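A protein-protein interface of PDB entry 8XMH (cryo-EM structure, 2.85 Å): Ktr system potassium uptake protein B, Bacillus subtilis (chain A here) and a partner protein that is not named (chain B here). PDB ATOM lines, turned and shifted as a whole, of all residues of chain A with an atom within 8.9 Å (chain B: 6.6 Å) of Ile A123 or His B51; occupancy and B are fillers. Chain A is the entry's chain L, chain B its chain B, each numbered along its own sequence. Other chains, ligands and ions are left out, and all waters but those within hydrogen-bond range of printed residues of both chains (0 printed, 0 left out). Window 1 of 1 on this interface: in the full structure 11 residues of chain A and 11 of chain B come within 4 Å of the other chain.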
ATOM      1  N   GLY A 107     -19.419   6.248 -23.511  1.00  0.00           N
ATOM      2  CA  GLY A 107     -19.240   6.149 -22.081  1.00  0.00           C
ATOM      3  C   GLY A 107     -20.375   5.416 -21.404  1.00  0.00           C
ATOM      4  O   GLY A 107     -21.313   4.929 -22.032  1.00  0.00           O
ATOM      5  N   LEU A 108     -20.266   5.320 -20.078  1.00  0.00           N
ATOM      6  CA  LEU A 108     -21.342   4.729 -19.291  1.00  0.00           C
ATOM      7  C   LEU A 108     -22.566   5.636 -19.268  1.00  0.00           C
ATOM      8  O   LEU A 108     -23.702   5.152 -19.315  1.00  0.00           O
ATOM      9  CB  LEU A 108     -20.857   4.440 -17.872  1.00  0.00           C
ATOM     10  CG  LEU A 108     -21.874   3.836 -16.905  1.00  0.00           C
ATOM     11  CD1 LEU A 108     -22.370   2.498 -17.418  1.00  0.00           C
ATOM     12  CD2 LEU A 108     -21.277   3.692 -15.520  1.00  0.00           C
ATOM     13  N   LYS A 109     -22.354   6.952 -19.187  1.00  0.00           N
ATOM     14  CA  LYS A 109     -23.472   7.890 -19.211  1.00  0.00           C
ATOM     15  C   LYS A 109     -24.195   7.857 -20.552  1.00  0.00           C
ATOM     16  O   LYS A 109     -25.429   7.915 -20.600  1.00  0.00           O
ATOM     17  CB  LYS A 109     -22.981   9.305 -18.912  1.00  0.00           C
ATOM     18  CG  LYS A 109     -22.315   9.464 -17.563  1.00  0.00           C
ATOM     19  CD  LYS A 109     -21.835  10.890 -17.355  1.00  0.00           C
ATOM     20  CE  LYS A 109     -21.016  11.015 -16.082  1.00  0.00           C
ATOM     21  NZ  LYS A 109     -20.463  12.387 -15.911  1.00  0.00           N
ATOM     22  N   GLU A 110     -23.443   7.771 -21.650  1.00  0.00           N
ATOM     23  CA  GLU A 110     -24.059   7.696 -22.969  1.00  0.00           C
ATOM     24  C   GLU A 110     -24.748   6.358 -23.188  1.00  0.00           C
ATOM     25  O   GLU A 110     -25.714   6.278 -23.955  1.00  0.00           O
ATOM     26  CB  GLU A 110     -23.007   7.934 -24.050  1.00  0.00           C
ATOM     27  CG  GLU A 110     -22.178   9.189 -23.832  1.00  0.00           C
ATOM     28  CD  GLU A 110     -21.066   9.342 -24.850  1.00  0.00           C
ATOM     29  OE1 GLU A 110     -20.881   8.420 -25.671  1.00  0.00           O
ATOM     30  OE2 GLU A 110     -20.378  10.384 -24.832  1.00  0.00           O
ATOM     31  N   ARG A 111     -24.267   5.302 -22.536  1.00  0.00           N
ATOM     32  CA  ARG A 111     -24.884   3.991 -22.680  1.00  0.00           C
ATOM     33  C   ARG A 111     -26.193   3.888 -21.910  1.00  0.00           C
ATOM     34  O   ARG A 111     -27.072   3.108 -22.292  1.00  0.00           O
ATOM     35  CB  ARG A 111     -23.911   2.908 -22.221  1.00  0.00           C
ATOM     36  CG  ARG A 111     -24.262   1.517 -22.699  1.00  0.00           C
ATOM     37  CD  ARG A 111     -23.166   0.522 -22.375  1.00  0.00           C
ATOM     38  NE  ARG A 111     -21.904   0.872 -23.015  1.00  0.00           N
ATOM     39  CZ  ARG A 111     -20.830   1.301 -22.368  1.00  0.00           C
ATOM     40  NH1 ARG A 111     -20.821   1.424 -21.051  1.00  0.00           N
ATOM     41  NH2 ARG A 111     -19.737   1.607 -23.059  1.00  0.00           N
ATOM     42  N   MET A 112     -26.343   4.657 -20.829  1.00  0.00           N
ATOM     43  CA  MET A 112     -27.595   4.645 -20.081  1.00  0.00           C
ATOM     44  C   MET A 112     -28.715   5.333 -20.850  1.00  0.00           C
ATOM     45  O   MET A 112     -29.890   5.008 -20.648  1.00  0.00           O
ATOM     46  CB  MET A 112     -27.402   5.307 -18.718  1.00  0.00           C
ATOM     47  CG  MET A 112     -26.509   4.522 -17.773  1.00  0.00           C
ATOM     48  SD  MET A 112     -26.134   5.410 -16.250  1.00  0.00           S
ATOM     49  CE  MET A 112     -27.764   5.535 -15.522  1.00  0.00           C
ATOM     50  N   LEU A 113     -28.378   6.287 -21.722  1.00  0.00           N
ATOM     51  CA  LEU A 113     -29.392   6.914 -22.564  1.00  0.00           C
ATOM     52  C   LEU A 113     -29.951   5.928 -23.581  1.00  0.00           C
ATOM     53  O   LEU A 113     -31.148   5.955 -23.884  1.00  0.00           O
ATOM     54  CB  LEU A 113     -28.805   8.130 -23.277  1.00  0.00           C
ATOM     55  CG  LEU A 113     -28.089   9.174 -22.422  1.00  0.00           C
ATOM     56  CD1 LEU A 113     -27.534  10.281 -23.300  1.00  0.00           C
ATOM     57  CD2 LEU A 113     -29.022   9.741 -21.374  1.00  0.00           C
ATOM     58  N   VAL A 114     -29.094   5.064 -24.126  1.00  0.00           N
ATOM     59  CA  VAL A 114     -29.540   4.056 -25.083  1.00  0.00           C
ATOM     60  C   VAL A 114     -30.449   3.040 -24.406  1.00  0.00           C
ATOM     61  O   VAL A 114     -31.404   2.538 -25.011  1.00  0.00           O
ATOM     62  CB  VAL A 114     -28.323   3.378 -25.734  1.00  0.00           C
ATOM     63  CG1 VAL A 114     -28.758   2.472 -26.865  1.00  0.00           C
ATOM     64  CG2 VAL A 114     -27.344   4.423 -26.226  1.00  0.00           C
ATOM     65  N   GLN A 115     -30.158   2.709 -23.147  1.00  0.00           N
ATOM     66  CA  GLN A 115     -31.004   1.782 -22.405  1.00  0.00           C
ATOM     67  C   GLN A 115     -32.404   2.350 -22.208  1.00  0.00           C
ATOM     68  O   GLN A 115     -33.399   1.626 -22.325  1.00  0.00           O
ATOM     69  CB  GLN A 115     -30.359   1.461 -21.059  1.00  0.00           C
ATOM     70  CG  GLN A 115     -31.081   0.404 -20.258  1.00  0.00           C
ATOM     71  CD  GLN A 115     -30.688   0.423 -18.800  1.00  0.00           C
ATOM     72  OE1 GLN A 115     -30.056   1.366 -18.328  1.00  0.00           O
ATOM     73  NE2 GLN A 115     -31.064  -0.621 -18.074  1.00  0.00           N
ATOM     74  N   GLU A 116     -32.501   3.647 -21.907  1.00  0.00           N
ATOM     75  CA  GLU A 116     -33.808   4.268 -21.715  1.00  0.00           C
ATOM     76  C   GLU A 116     -34.545   4.437 -23.038  1.00  0.00           C
ATOM     77  O   GLU A 116     -35.770   4.275 -23.096  1.00  0.00           O
ATOM     78  CB  GLU A 116     -33.643   5.616 -21.012  1.00  0.00           C
ATOM     79  CG  GLU A 116     -34.951   6.309 -20.657  1.00  0.00           C
ATOM     80  CD  GLU A 116     -35.706   5.612 -19.540  1.00  0.00           C
ATOM     81  OE1 GLU A 116     -35.068   4.898 -18.737  1.00  0.00           O
ATOM     82  OE2 GLU A 116     -36.942   5.779 -19.465  1.00  0.00           O
ATOM     83  N   GLN A 120     -34.831  -0.909 -22.628  1.00  0.00           N
ATOM     84  CA  GLN A 120     -34.128  -2.117 -22.231  1.00  0.00           C
ATOM     85  C   GLN A 120     -34.025  -2.201 -20.711  1.00  0.00           C
ATOM     86  O   GLN A 120     -33.947  -1.175 -20.029  1.00  0.00           O
ATOM     87  CB  GLN A 120     -32.731  -2.140 -22.843  1.00  0.00           C
ATOM     88  CG  GLN A 120     -32.402  -3.418 -23.591  1.00  0.00           C
ATOM     89  CD  GLN A 120     -33.337  -3.670 -24.757  1.00  0.00           C
ATOM     90  OE1 GLN A 120     -33.764  -2.740 -25.441  1.00  0.00           O
ATOM     91  NE2 GLN A 120     -33.662  -4.935 -24.989  1.00  0.00           N
ATOM     92  N   PRO A 121     -34.033  -3.414 -20.148  1.00  0.00           N
ATOM     93  CA  PRO A 121     -33.859  -3.541 -18.694  1.00  0.00           C
ATOM     94  C   PRO A 121     -32.411  -3.495 -18.242  1.00  0.00           C
ATOM     95  O   PRO A 121     -32.157  -3.121 -17.090  1.00  0.00           O
ATOM     96  CB  PRO A 121     -34.486  -4.906 -18.387  1.00  0.00           C
ATOM     97  CG  PRO A 121     -34.268  -5.686 -19.638  1.00  0.00           C
ATOM     98  CD  PRO A 121     -34.370  -4.702 -20.777  1.00  0.00           C
ATOM     99  N   THR A 122     -31.462  -3.862 -19.100  1.00  0.00           N
ATOM    100  CA  THR A 122     -30.049  -3.890 -18.755  1.00  0.00           C
ATOM    101  C   THR A 122     -29.240  -3.225 -19.859  1.00  0.00           C
ATOM    102  O   THR A 122     -29.685  -3.117 -21.004  1.00  0.00           O
ATOM    103  CB  THR A 122     -29.547  -5.325 -18.535  1.00  0.00           C
ATOM    104  OG1 THR A 122     -29.899  -6.135 -19.665  1.00  0.00           O
ATOM    105  CG2 THR A 122     -30.150  -5.927 -17.273  1.00  0.00           C
ATOM    106  N   ILE A 123     -28.033  -2.781 -19.503  1.00  0.00           N
ATOM    107  CA  ILE A 123     -27.141  -2.128 -20.455  1.00  0.00           C
ATOM    108  C   ILE A 123     -26.219  -3.159 -21.090  1.00  0.00           C
ATOM    109  O   ILE A 123     -25.232  -2.808 -21.745  1.00  0.00           O
ATOM    110  CB  ILE A 123     -26.322  -1.006 -19.788  1.00  0.00           C
ATOM    111  CG1 ILE A 123     -25.626  -1.527 -18.531  1.00  0.00           C
ATOM    112  CG2 ILE A 123     -27.203   0.182 -19.462  1.00  0.00           C
ATOM    113  CD1 ILE A 123     -24.803  -0.478 -17.815  1.00  0.00           C
ATOM    114  N   GLY A 124     -26.532  -4.436 -20.901  1.00  0.00           N
ATOM    115  CA  GLY A 124     -25.730  -5.496 -21.477  1.00  0.00           C
ATOM    116  C   GLY A 124     -25.954  -5.671 -22.963  1.00  0.00           C
ATOM    117  O   GLY A 124     -27.020  -6.125 -23.388  1.00  0.00           O
ATOM    118  N   GLY A 125     -24.951  -5.321 -23.761  1.00  0.00           N
ATOM    119  CA  GLY A 125     -25.043  -5.458 -25.203  1.00  0.00           C
ATOM    120  C   GLY A 125     -26.078  -4.569 -25.856  1.00  0.00           C
ATOM    121  O   GLY A 125     -26.793  -5.018 -26.761  1.00  0.00           O
ATOM    122  N   VAL A 126     -26.178  -3.315 -25.421  1.00  0.00           N
ATOM    123  CA  VAL A 126     -27.144  -2.392 -26.001  1.00  0.00           C
ATOM    124  C   VAL A 126     -26.523  -1.495 -27.071  1.00  0.00           C
ATOM    125  O   VAL A 126     -27.245  -1.027 -27.965  1.00  0.00           O
ATOM    126  CB  VAL A 126     -27.825  -1.550 -24.896  1.00  0.00           C
ATOM    127  CG1 VAL A 126     -26.907  -0.455 -24.377  1.00  0.00           C
ATOM    128  CG2 VAL A 126     -29.151  -0.981 -25.377  1.00  0.00           C
ATOM    129  N   ILE A 127     -25.209  -1.260 -27.026  1.00  0.00           N
ATOM    130  CA  ILE A 127     -24.551  -0.508 -28.088  1.00  0.00           C
ATOM    131  C   ILE A 127     -24.476  -1.341 -29.362  1.00  0.00           C
ATOM    132  O   ILE A 127     -24.674  -0.829 -30.470  1.00  0.00           O
ATOM    133  CB  ILE A 127     -23.160  -0.036 -27.627  1.00  0.00           C
ATOM    134  CG1 ILE A 127     -23.296   0.905 -26.432  1.00  0.00           C
ATOM    135  CG2 ILE A 127     -22.424   0.670 -28.752  1.00  0.00           C
ATOM    136  CD1 ILE A 127     -24.162   2.110 -26.711  1.00  0.00           C
ATOM    137  N   GLY A 128     -24.198  -2.640 -29.226  1.00  0.00           N
ATOM    138  CA  GLY A 128     -24.174  -3.517 -30.381  1.00  0.00           C
ATOM    139  C   GLY A 128     -25.530  -3.733 -31.016  1.00  0.00           C
ATOM    140  O   GLY A 128     -25.600  -4.062 -32.203  1.00  0.00           O
ATOM    141  N   LEU A 129     -26.608  -3.561 -30.250  1.00  0.00           N
ATOM    142  CA  LEU A 129     -27.949  -3.649 -30.818  1.00  0.00           C
ATOM    143  C   LEU A 129     -28.221  -2.491 -31.772  1.00  0.00           C
ATOM    144  O   LEU A 129     -28.901  -2.666 -32.789  1.00  0.00           O
ATOM    145  CB  LEU A 129     -28.989  -3.684 -29.699  1.00  0.00           C
ATOM    146  CG  LEU A 129     -30.464  -3.770 -30.092  1.00  0.00           C
ATOM    147  CD1 LEU A 129     -30.746  -5.048 -30.863  1.00  0.00           C
ATOM    148  CD2 LEU A 129     -31.343  -3.682 -28.857  1.00  0.00           C
ATOM    149  N   GLU B  31     -16.467   8.083 -14.571  1.00  0.00           N
ATOM    150  CA  GLU B  31     -17.635   7.223 -14.728  1.00  0.00           C
ATOM    151  C   GLU B  31     -17.404   5.941 -13.942  1.00  0.00           C
ATOM    152  O   GLU B  31     -16.553   5.127 -14.305  1.00  0.00           O
ATOM    153  CB  GLU B  31     -17.889   6.926 -16.202  1.00  0.00           C
ATOM    154  CG  GLU B  31     -18.237   8.151 -17.027  1.00  0.00           C
ATOM    155  CD  GLU B  31     -18.293   7.859 -18.513  1.00  0.00           C
ATOM    156  OE1 GLU B  31     -17.907   6.743 -18.917  1.00  0.00           O
ATOM    157  OE2 GLU B  31     -18.721   8.748 -19.279  1.00  0.00           O
ATOM    158  N   VAL B  32     -18.164   5.759 -12.867  1.00  0.00           N
ATOM    159  CA  VAL B  32     -17.994   4.638 -11.953  1.00  0.00           C
ATOM    160  C   VAL B  32     -19.259   3.796 -11.975  1.00  0.00           C
ATOM    161  O   VAL B  32     -20.364   4.325 -11.821  1.00  0.00           O
ATOM    162  CB  VAL B  32     -17.688   5.113 -10.521  1.00  0.00           C
ATOM    163  CG1 VAL B  32     -17.303   3.937  -9.648  1.00  0.00           C
ATOM    164  CG2 VAL B  32     -16.592   6.148 -10.531  1.00  0.00           C
ATOM    165  N   LEU B  33     -19.097   2.492 -12.166  1.00  0.00           N
ATOM    166  CA  LEU B  33     -20.184   1.539 -12.008  1.00  0.00           C
ATOM    167  C   LEU B  33     -20.018   0.848 -10.661  1.00  0.00           C
ATOM    168  O   LEU B  33     -19.002   0.190 -10.419  1.00  0.00           O
ATOM    169  CB  LEU B  33     -20.190   0.517 -13.142  1.00  0.00           C
ATOM    170  CG  LEU B  33     -21.197  -0.625 -13.000  1.00  0.00           C
ATOM    171  CD1 LEU B  33     -22.610  -0.101 -13.088  1.00  0.00           C
ATOM    172  CD2 LEU B  33     -20.957  -1.692 -14.042  1.00  0.00           C
ATOM    173  N   ALA B  34     -21.006   1.001  -9.791  1.00  0.00           N
ATOM    174  CA  ALA B  34     -20.978   0.409  -8.462  1.00  0.00           C
ATOM    175  C   ALA B  34     -21.868  -0.824  -8.452  1.00  0.00           C
ATOM    176  O   ALA B  34     -23.079  -0.722  -8.660  1.00  0.00           O
ATOM    177  CB  ALA B  34     -21.443   1.414  -7.411  1.00  0.00           C
ATOM    178  N   VAL B  35     -21.269  -1.985  -8.207  1.00  0.00           N
ATOM    179  CA  VAL B  35     -21.979  -3.256  -8.204  1.00  0.00           C
ATOM    180  C   VAL B  35     -21.891  -3.845  -6.806  1.00  0.00           C
ATOM    181  O   VAL B  35     -20.803  -3.917  -6.226  1.00  0.00           O
ATOM    182  CB  VAL B  35     -21.404  -4.235  -9.242  1.00  0.00           C
ATOM    183  CG1 VAL B  35     -22.304  -5.443  -9.375  1.00  0.00           C
ATOM    184  CG2 VAL B  35     -21.220  -3.551 -10.581  1.00  0.00           C
ATOM    185  N   TYR B  45     -25.110   4.160  -2.155  1.00  0.00           N
ATOM    186  CA  TYR B  45     -24.096   4.624  -3.092  1.00  0.00           C
ATOM    187  C   TYR B  45     -24.664   4.941  -4.467  1.00  0.00           C
ATOM    188  O   TYR B  45     -23.894   5.112  -5.416  1.00  0.00           O
ATOM    189  CB  TYR B  45     -22.974   3.592  -3.215  1.00  0.00           C
ATOM    190  CG  TYR B  45     -22.098   3.510  -1.987  1.00  0.00           C
ATOM    191  CD1 TYR B  45     -21.056   4.404  -1.796  1.00  0.00           C
ATOM    192  CD2 TYR B  45     -22.318   2.545  -1.018  1.00  0.00           C
ATOM    193  CE1 TYR B  45     -20.262   4.341  -0.675  1.00  0.00           C
ATOM    194  CE2 TYR B  45     -21.527   2.470   0.106  1.00  0.00           C
ATOM    195  CZ  TYR B  45     -20.500   3.370   0.272  1.00  0.00           C
ATOM    196  OH  TYR B  45     -19.708   3.296   1.395  1.00  0.00           O
ATOM    197  N   ALA B  46     -25.989   5.008  -4.599  1.00  0.00           N
ATOM    198  CA  ALA B  46     -26.588   5.382  -5.875  1.00  0.00           C
ATOM    199  C   ALA B  46     -26.247   6.818  -6.247  1.00  0.00           C
ATOM    200  O   ALA B  46     -26.023   7.124  -7.423  1.00  0.00           O
ATOM    201  CB  ALA B  46     -28.102   5.184  -5.823  1.00  0.00           C
ATOM    202  N   ALA B  49     -22.269   7.280  -7.320  1.00  0.00           N
ATOM    203  CA  ALA B  49     -21.763   6.564  -8.478  1.00  0.00           C
ATOM    204  C   ALA B  49     -22.553   6.983  -9.706  1.00  0.00           C
ATOM    205  O   ALA B  49     -23.709   7.401  -9.606  1.00  0.00           O
ATOM    206  CB  ALA B  49     -21.854   5.047  -8.291  1.00  0.00           C
ATOM    207  N   THR B  50     -21.911   6.878 -10.870  1.00  0.00           N
ATOM    208  CA  THR B  50     -22.602   7.160 -12.122  1.00  0.00           C
ATOM    209  C   THR B  50     -23.732   6.165 -12.356  1.00  0.00           C
ATOM    210  O   THR B  50     -24.838   6.549 -12.755  1.00  0.00           O
ATOM    211  CB  THR B  50     -21.608   7.133 -13.282  1.00  0.00           C
ATOM    212  OG1 THR B  50     -20.605   8.133 -13.072  1.00  0.00           O
ATOM    213  CG2 THR B  50     -22.309   7.405 -14.597  1.00  0.00           C
ATOM    214  N   HIS B  51     -23.479   4.888 -12.091  1.00  0.00           N
ATOM    215  CA  HIS B  51     -24.481   3.842 -12.227  1.00  0.00           C
ATOM    216  C   HIS B  51     -24.285   2.840 -11.103  1.00  0.00           C
ATOM    217  O   HIS B  51     -23.163   2.388 -10.866  1.00  0.00           O
ATOM    218  CB  HIS B  51     -24.372   3.150 -13.587  1.00  0.00           C
ATOM    219  CG  HIS B  51     -25.523   2.248 -13.900  1.00  0.00           C
ATOM    220  ND1 HIS B  51     -25.479   1.306 -14.905  1.00  0.00           N
ATOM    221  CD2 HIS B  51     -26.753   2.151 -13.346  1.00  0.00           C
ATOM    222  CE1 HIS B  51     -26.631   0.664 -14.953  1.00  0.00           C
ATOM    223  NE2 HIS B  51     -27.423   1.157 -14.017  1.00  0.00           N
ATOM    224  N   ALA B  52     -25.367   2.503 -10.407  1.00  0.00           N
ATOM    225  CA  ALA B  52     -25.334   1.545  -9.312  1.00  0.00           C
ATOM    226  C   ALA B  52     -26.312   0.419  -9.606  1.00  0.00           C
ATOM    227  O   ALA B  52     -27.488   0.673  -9.876  1.00  0.00           O
ATOM    228  CB  ALA B  52     -25.674   2.217  -7.983  1.00  0.00           C
ATOM    229  N   VAL B  53     -25.825  -0.819  -9.565  1.00  0.00           N
ATOM    230  CA  VAL B  53     -26.606  -1.992  -9.937  1.00  0.00           C
ATOM    231  C   VAL B  53     -26.550  -3.007  -8.804  1.00  0.00           C
ATOM    232  O   VAL B  53     -25.489  -3.227  -8.211  1.00  0.00           O
ATOM    233  CB  VAL B  53     -26.099  -2.631 -11.248  1.00  0.00           C
ATOM    234  CG1 VAL B  53     -27.052  -3.709 -11.717  1.00  0.00           C
ATOM    235  CG2 VAL B  53     -25.923  -1.587 -12.331  1.00  0.00           C
ATOM    236  N   LEU B  64     -22.527 -10.004 -17.655  1.00  0.00           N
ATOM    237  CA  LEU B  64     -22.646  -9.537 -19.032  1.00  0.00           C
ATOM    238  C   LEU B  64     -23.796  -8.557 -19.216  1.00  0.00           C
ATOM    239  O   LEU B  64     -23.797  -7.800 -20.191  1.00  0.00           O
ATOM    240  CB  LEU B  64     -22.817 -10.724 -19.978  1.00  0.00           C
ATOM    241  CG  LEU B  64     -21.587 -11.606 -20.173  1.00  0.00           C
ATOM    242  CD1 LEU B  64     -21.914 -12.786 -21.065  1.00  0.00           C
ATOM    243  CD2 LEU B  64     -20.448 -10.794 -20.756  1.00  0.00           C
ATOM    244  N   SER B  65     -24.774  -8.555 -18.309  1.00  0.00           N
ATOM    245  CA  SER B  65     -25.868  -7.598 -18.395  1.00  0.00           C
ATOM    246  C   SER B  65     -25.439  -6.194 -17.994  1.00  0.00           C
ATOM    247  O   SER B  65     -26.145  -5.232 -18.306  1.00  0.00           O
ATOM    248  CB  SER B  65     -27.032  -8.050 -17.516  1.00  0.00           C
ATOM    249  OG  SER B  65     -27.459  -9.351 -17.877  1.00  0.00           O
ATOM    250  N   LEU B  66     -24.308  -6.057 -17.307  1.00  0.00           N
ATOM    251  CA  LEU B  66     -23.797  -4.758 -16.898  1.00  0.00           C
ATOM    252  C   LEU B  66     -22.977  -4.077 -17.979  1.00  0.00           C
ATOM    253  O   LEU B  66     -22.619  -2.907 -17.816  1.00  0.00           O
ATOM    254  CB  LEU B  66     -22.925  -4.894 -15.646  1.00  0.00           C
ATOM    255  CG  LEU B  66     -23.404  -5.801 -14.521  1.00  0.00           C
ATOM    256  CD1 LEU B  66     -22.395  -5.812 -13.391  1.00  0.00           C
ATOM    257  CD2 LEU B  66     -24.754  -5.347 -14.031  1.00  0.00           C
ATOM    258  N   GLY B  67     -22.678  -4.769 -19.072  1.00  0.00           N
ATOM    259  CA  GLY B  67     -21.723  -4.249 -20.029  1.00  0.00           C
ATOM    260  C   GLY B  67     -20.335  -4.143 -19.439  1.00  0.00           C
ATOM    261  O   GLY B  67     -19.645  -3.142 -19.662  1.00  0.00           O
ATOM    262  N   ILE B  68     -19.911  -5.158 -18.682  1.00  0.00           N
ATOM    263  CA  ILE B  68     -18.645  -5.094 -17.963  1.00  0.00           C
ATOM    264  C   ILE B  68     -17.452  -5.162 -18.907  1.00  0.00           C
ATOM    265  O   ILE B  68     -16.333  -4.827 -18.508  1.00  0.00           O
ATOM    266  CB  ILE B  68     -18.590  -6.218 -16.908  1.00  0.00           C
ATOM    267  CG1 ILE B  68     -17.620  -5.869 -15.779  1.00  0.00           C
ATOM    268  CG2 ILE B  68     -18.209  -7.532 -17.548  1.00  0.00           C
ATOM    269  CD1 ILE B  68     -18.134  -4.806 -14.848  1.00  0.00           C
ATOM    270  N   ASN B  70     -16.943  -3.174 -21.255  1.00  0.00           N
ATOM    271  CA  ASN B  70     -16.657  -1.806 -21.662  1.00  0.00           C
ATOM    272  C   ASN B  70     -15.817  -1.046 -20.646  1.00  0.00           C
ATOM    273  O   ASN B  70     -15.546   0.141 -20.854  1.00  0.00           O
ATOM    274  CB  ASN B  70     -17.967  -1.054 -21.910  1.00  0.00           C
ATOM    275  CG  ASN B  70     -18.834  -1.725 -22.953  1.00  0.00           C
ATOM    276  OD1 ASN B  70     -19.936  -2.185 -22.659  1.00  0.00           O
ATOM    277  ND2 ASN B  70     -18.338  -1.786 -24.183  1.00  0.00           N
ATOM    278  N   PHE B  71     -15.400  -1.690 -19.561  1.00  0.00           N
ATOM    279  CA  PHE B  71     -14.645  -1.045 -18.498  1.00  0.00           C
ATOM    280  C   PHE B  71     -13.187  -1.470 -18.572  1.00  0.00           C
ATOM    281  O   PHE B  71     -12.888  -2.667 -18.638  1.00  0.00           O
ATOM    282  CB  PHE B  71     -15.232  -1.386 -17.130  1.00  0.00           C
ATOM    283  CG  PHE B  71     -16.621  -0.867 -16.929  1.00  0.00           C
ATOM    284  CD1 PHE B  71     -16.833   0.423 -16.487  1.00  0.00           C
ATOM    285  CD2 PHE B  71     -17.716  -1.663 -17.192  1.00  0.00           C
ATOM    286  CE1 PHE B  71     -18.107   0.908 -16.308  1.00  0.00           C
ATOM    287  CE2 PHE B  71     -18.992  -1.184 -17.015  1.00  0.00           C
ATOM    288  CZ  PHE B  71     -19.186   0.104 -16.573  1.00  0.00           C
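N of Ile A123 is in hydrogen-bond range of O of Ser B65, 3.3 Å away.
O of Ser B65 is in hydrogen-bond range of N of Gly A124 (2.7 Å).
OE1 of Glu B31 lies within hydrogen-bond range of N of Leu A108 (3.0 Å).
OE1 of Glu A110 is in hydrogen-bond range of N of Gly A107 (3.4 Å).
The backbone NH (N) of Thr B50 is in hydrogen-bond range of the backbone carbonyl oxygen (O) of Val B32 (3.1 Å).
The backbone NH of Ala B34 is in hydrogen-bond range of the backbone carbonyl oxygen of His B51.
The backbone carbonyl oxygen (O) of Val B32 sits at hydrogen-bond distance from the backbone NH (N) of His B51, at 3.2 Å.
The side-chain amide oxygen (OD1) of Asn B70 sits close to the backbone carbonyl oxygen (O) of Gly B67, at 3.2 Å.
The backbone NH (N) of Thr A122 sits close to the side-chain amide nitrogen (NE2) of Gln A115 (3.4 Å).
CA of Gly A107 touches OE1 of Glu B31, 3.5 Å away.
O of Val B32 touches CD2 of Leu A108 (3.9 Å).
Leu A108 touches His B51.
Lys A109 touches Thr B50.
Met A112 touches Thr B50.
CB of His B51 touches SD of Met A112 (3.9 Å).
His B51 touches Ile A123 (ND1 to CD1, 3.5 Å).
Ile A123 touches Leu B66 (CD1 to O, 3.3 Å).
CA of Gly A124 touches O of Leu B64, at 3.3 Å.
Gly B67 touches Gly A124 (N to CA, 3.95 Å).
Printed residues of chain B within 4 Å of Arg A111: Asn B70 (3.4 Å).
Of the printed residues of chain A, Glu B31 touches Gly A107 and Leu A108.
No residue of chain A comes within 4 Å of Ala B34.
Thr B50 touches just these residues of chain A: Leu A108, Lys A109 and Met A112.
Of chain A, only Leu A108, Met A112 and Ile A123 come within 4 Å of His B51.
No residue of chain A comes within 4 Å of Ala B52.
Printed residues of chain A within 4 Å of Ser B65: Thr A122, Ile A123 and Gly A124.
Of the printed residues of chain A, Leu B66 touches Ile A123.
The nearest printed residue of chain A that does not touch Leu B66 is Gly A124 (4.4 Å).
Printed residues of chain A that touch a printed residue of chain B: Gly A107, Leu A108, Lys A109, Arg A111, Met A112, Thr A122, Ile A123 and Gly A124.
Along chain A the printed residues that touch a printed residue of chain B span positions 107 to 124.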
